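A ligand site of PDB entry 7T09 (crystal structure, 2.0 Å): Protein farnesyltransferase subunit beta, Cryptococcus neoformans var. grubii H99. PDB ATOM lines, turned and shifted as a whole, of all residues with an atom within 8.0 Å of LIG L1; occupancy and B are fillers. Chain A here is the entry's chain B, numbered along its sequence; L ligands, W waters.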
ATOM      1  N   LEU A  50      -0.508  18.790  10.158  1.00  0.00           N
ATOM      2  CA  LEU A  50      -0.273  20.226  10.115  1.00  0.00           C
ATOM      3  C   LEU A  50       0.982  20.626  10.873  1.00  0.00           C
ATOM      4  O   LEU A  50       1.623  21.637  10.536  1.00  0.00           O
ATOM      5  CB  LEU A  50      -1.469  20.974  10.697  1.00  0.00           C
ATOM      6  CG  LEU A  50      -2.840  20.373  10.385  1.00  0.00           C
ATOM      7  CD1 LEU A  50      -3.922  21.085  11.182  1.00  0.00           C
ATOM      8  CD2 LEU A  50      -3.132  20.427   8.894  1.00  0.00           C
ATOM      9  N   TYR A  58      10.124  17.761   4.110  1.00  0.00           N
ATOM     10  CA  TYR A  58       8.785  18.169   3.692  1.00  0.00           C
ATOM     11  C   TYR A  58       8.476  17.561   2.330  1.00  0.00           C
ATOM     12  O   TYR A  58       9.261  17.698   1.389  1.00  0.00           O
ATOM     13  CB  TYR A  58       8.665  19.702   3.635  1.00  0.00           C
ATOM     14  CG  TYR A  58       7.303  20.139   3.132  1.00  0.00           C
ATOM     15  CD1 TYR A  58       7.156  20.909   1.979  1.00  0.00           C
ATOM     16  CD2 TYR A  58       6.154  19.724   3.795  1.00  0.00           C
ATOM     17  CE1 TYR A  58       5.886  21.270   1.505  1.00  0.00           C
ATOM     18  CE2 TYR A  58       4.893  20.077   3.347  1.00  0.00           C
ATOM     19  CZ  TYR A  58       4.750  20.842   2.206  1.00  0.00           C
ATOM     20  OH  TYR A  58       3.478  21.166   1.776  1.00  0.00           O
ATOM     21  N   GLY A  60       5.928  18.113   0.116  1.00  0.00           N
ATOM     22  CA  GLY A  60       5.154  18.815  -0.892  1.00  0.00           C
ATOM     23  C   GLY A  60       5.649  18.607  -2.319  1.00  0.00           C
ATOM     24  O   GLY A  60       6.854  18.451  -2.556  1.00  0.00           O
ATOM     25  N   LEU A  61       4.723  18.585  -3.272  1.00  0.00           N
ATOM     26  CA  LEU A  61       5.083  18.376  -4.674  1.00  0.00           C
ATOM     27  C   LEU A  61       5.940  19.525  -5.176  1.00  0.00           C
ATOM     28  O   LEU A  61       5.499  20.694  -5.186  1.00  0.00           O
ATOM     29  CB  LEU A  61       3.814  18.243  -5.519  1.00  0.00           C
ATOM     30  CG  LEU A  61       4.029  17.874  -6.994  1.00  0.00           C
ATOM     31  CD1 LEU A  61       4.641  16.472  -7.116  1.00  0.00           C
ATOM     32  CD2 LEU A  61       2.710  17.957  -7.772  1.00  0.00           C
ATOM     33  N   ILE A 486      -6.944  15.597  -2.107  1.00  0.00           N
ATOM     34  CA  ILE A 486      -5.611  16.156  -2.354  1.00  0.00           C
ATOM     35  C   ILE A 486      -4.788  15.987  -1.090  1.00  0.00           C
ATOM     36  O   ILE A 486      -4.835  16.837  -0.190  1.00  0.00           O
ATOM     37  CB  ILE A 486      -5.664  17.629  -2.778  1.00  0.00           C
ATOM     38  CG1 ILE A 486      -6.759  17.889  -3.820  1.00  0.00           C
ATOM     39  CG2 ILE A 486      -4.296  18.064  -3.315  1.00  0.00           C
ATOM     40  CD1 ILE A 486      -6.550  17.129  -5.141  1.00  0.00           C
ATOM     41  N   VAL A 487      -3.998  14.910  -1.024  1.00  0.00           N
ATOM     42  CA  VAL A 487      -3.159  14.649   0.148  1.00  0.00           C
ATOM     43  C   VAL A 487      -2.124  15.758   0.294  1.00  0.00           C
ATOM     44  O   VAL A 487      -1.464  16.159  -0.672  1.00  0.00           O
ATOM     45  CB  VAL A 487      -2.478  13.276   0.028  1.00  0.00           C
ATOM     46  CG1 VAL A 487      -1.445  13.063   1.155  1.00  0.00           C
ATOM     47  CG2 VAL A 487      -3.513  12.164   0.062  1.00  0.00           C
ATOM     48  N   GLY A 488      -1.991  16.269   1.520  1.00  0.00           N
ATOM     49  CA  GLY A 488      -0.983  17.277   1.814  1.00  0.00           C
ATOM     50  C   GLY A 488      -1.375  18.718   1.548  1.00  0.00           C
ATOM     51  O   GLY A 488      -0.548  19.619   1.760  1.00  0.00           O
ATOM     52  N   GLY A 489      -2.600  18.976   1.078  1.00  0.00           N
ATOM     53  CA  GLY A 489      -3.062  20.326   0.893  1.00  0.00           C
ATOM     54  C   GLY A 489      -3.191  20.683  -0.587  1.00  0.00           C
ATOM     55  O   GLY A 489      -2.615  20.038  -1.480  1.00  0.00           O
ATOM     56  N   LYS A 490      -3.939  21.762  -0.848  1.00  0.00           N
ATOM     57  CA  LYS A 490      -4.329  22.091  -2.213  1.00  0.00           C
ATOM     58  C   LYS A 490      -3.150  22.495  -3.095  1.00  0.00           C
ATOM     59  O   LYS A 490      -3.275  22.402  -4.317  1.00  0.00           O
ATOM     60  CB  LYS A 490      -5.410  23.167  -2.191  1.00  0.00           C
ATOM     61  CG  LYS A 490      -6.738  22.644  -1.635  1.00  0.00           C
ATOM     62  CD  LYS A 490      -7.888  23.621  -1.826  1.00  0.00           C
ATOM     63  CE  LYS A 490      -9.173  23.097  -1.199  1.00  0.00           C
ATOM     64  NZ  LYS A 490     -10.151  24.199  -0.929  1.00  0.00           N
ATOM     65  N   ASP A 491      -2.023  22.929  -2.524  1.00  0.00           N
ATOM     66  CA  ASP A 491      -0.889  23.231  -3.377  1.00  0.00           C
ATOM     67  C   ASP A 491      -0.307  21.987  -4.040  1.00  0.00           C
ATOM     68  O   ASP A 491       0.521  22.120  -4.960  1.00  0.00           O
ATOM     69  CB  ASP A 491       0.222  23.950  -2.594  1.00  0.00           C
ATOM     70  CG  ASP A 491      -0.127  25.411  -2.271  1.00  0.00           C
ATOM     71  OD1 ASP A 491      -0.667  26.116  -3.165  1.00  0.00           O
ATOM     72  OD2 ASP A 491       0.133  25.850  -1.130  1.00  0.00           O
ATOM     73  N   ASN A 492      -0.694  20.787  -3.613  1.00  0.00           N
ATOM     74  CA  ASN A 492      -0.294  19.560  -4.292  1.00  0.00           C
ATOM     75  C   ASN A 492      -1.189  19.197  -5.473  1.00  0.00           C
ATOM     76  O   ASN A 492      -0.868  18.247  -6.197  1.00  0.00           O
ATOM     77  CB  ASN A 492      -0.244  18.367  -3.325  1.00  0.00           C
ATOM     78  CG  ASN A 492       0.900  18.450  -2.327  1.00  0.00           C
ATOM     79  OD1 ASN A 492       1.868  19.190  -2.533  1.00  0.00           O
ATOM     80  ND2 ASN A 492       0.806  17.684  -1.252  1.00  0.00           N
ATOM     81  N   ARG A 493      -2.307  19.887  -5.663  1.00  0.00           N
ATOM     82  CA  ARG A 493      -3.258  19.510  -6.710  1.00  0.00           C
ATOM     83  C   ARG A 493      -2.630  19.638  -8.103  1.00  0.00           C
ATOM     84  O   ARG A 493      -1.957  20.625  -8.397  1.00  0.00           O
ATOM     85  CB  ARG A 493      -4.518  20.375  -6.633  1.00  0.00           C
ATOM     86  CG  ARG A 493      -5.574  20.006  -7.672  1.00  0.00           C
ATOM     87  CD  ARG A 493      -6.449  21.210  -8.019  1.00  0.00           C
ATOM     88  NE  ARG A 493      -7.485  20.847  -8.984  1.00  0.00           N
ATOM     89  CZ  ARG A 493      -7.388  20.996 -10.300  1.00  0.00           C
ATOM     90  NH1 ARG A 493      -6.293  21.517 -10.861  1.00  0.00           N
ATOM     91  NH2 ARG A 493      -8.402  20.615 -11.066  1.00  0.00           N
HETATM   92  O1  LIG L   1      -5.998  24.715   2.882  1.00  0.00           O
HETATM   93  O2  LIG L   1      -5.075  22.838   1.570  1.00  0.00           O
HETATM   94  O3  LIG L   1      -2.383  24.501   0.171  1.00  0.00           O
HETATM   95  O4  LIG L   1      -5.373  25.131   0.690  1.00  0.00           O
HETATM   96  C1  LIG L   1       4.051  26.449   1.731  1.00  0.00           C
HETATM   97  C2  LIG L   1       2.912  26.965   2.632  1.00  0.00           C
HETATM   98  C3  LIG L   1       3.954  24.940   1.464  1.00  0.00           C
HETATM   99  C4  LIG L   1       1.521  26.537   2.141  1.00  0.00           C
HETATM  100  C5  LIG L   1       2.582  24.563   0.896  1.00  0.00           C
HETATM  101  C6  LIG L   1      -0.889  25.047   2.042  1.00  0.00           C
HETATM  102  C7  LIG L   1      -3.272  24.593   2.478  1.00  0.00           C
HETATM  103  N1  LIG L   1       0.176  24.801   1.085  1.00  0.00           N
HETATM  104  C8  LIG L   1      -2.293  25.122   1.433  1.00  0.00           C
HETATM  105  C9  LIG L   1       1.435  25.039   1.787  1.00  0.00           C
HETATM  106  S1  LIG L   1      -4.961  24.299   1.886  1.00  0.00           S
HETATM  107  O1  LG2 L   2      10.421  22.976  -4.495  1.00  0.00           O
HETATM  108  O2  LG2 L   2       9.619  23.082  -6.819  1.00  0.00           O
HETATM  109  O3  LG2 L   2      12.107  24.897  -3.978  1.00  0.00           O
HETATM  110  O4  LG2 L   2       8.449  24.220  -4.950  1.00  0.00           O
HETATM  111  C1  LG2 L   2      13.432  31.104  -2.288  1.00  0.00           C
HETATM  112  C2  LG2 L   2      14.655  30.201  -2.389  1.00  0.00           C
HETATM  113  C3  LG2 L   2      12.520  30.979  -3.509  1.00  0.00           C
HETATM  114  C4  LG2 L   2      14.294  28.745  -2.702  1.00  0.00           C
HETATM  115  C5  LG2 L   2      12.128  29.529  -3.762  1.00  0.00           C
HETATM  116  C6  LG2 L   2      12.722  26.772  -5.315  1.00  0.00           C
HETATM  117  C7  LG2 L   2      10.713  25.407  -5.861  1.00  0.00           C
HETATM  118  N1  LG2 L   2      12.866  27.218  -3.941  1.00  0.00           N
HETATM  119  C8  LG2 L   2      12.135  25.354  -5.307  1.00  0.00           C
HETATM  120  C9  LG2 L   2      13.340  28.612  -3.887  1.00  0.00           C
HETATM  121  S1  LG2 L   2       9.787  23.871  -5.551  1.00  0.00           S
HETATM  122  O   HOH W   1      -5.637  26.173   5.573  1.00  0.00           O
HETATM  123  O   HOH W   2      -0.035  21.924   0.336  1.00  0.00           O
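The backbone NH (N) of Asp 491 lies within hydrogen-bond range of an oxygen (O3) of LIG L1, at 3.1 Å. The side-chain carboxylate of Asp 491 is in salt-bridge range of a nitrogen (N1) of LIG L1 (2.5 Å). The backbone NH of Lys 490 lies within hydrogen-bond range of an oxygen (O2) of LIG L1, at 2.9 Å.
Tyr 58 touches LIG L1. CA of Gly 489 touches O2 of LIG L1, at 3.3 Å. Of the 12 residues printed, 4 come within 4 Å of LIG L1.
Water W2 bridges O of Gly 488 and N1 of LIG L1.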
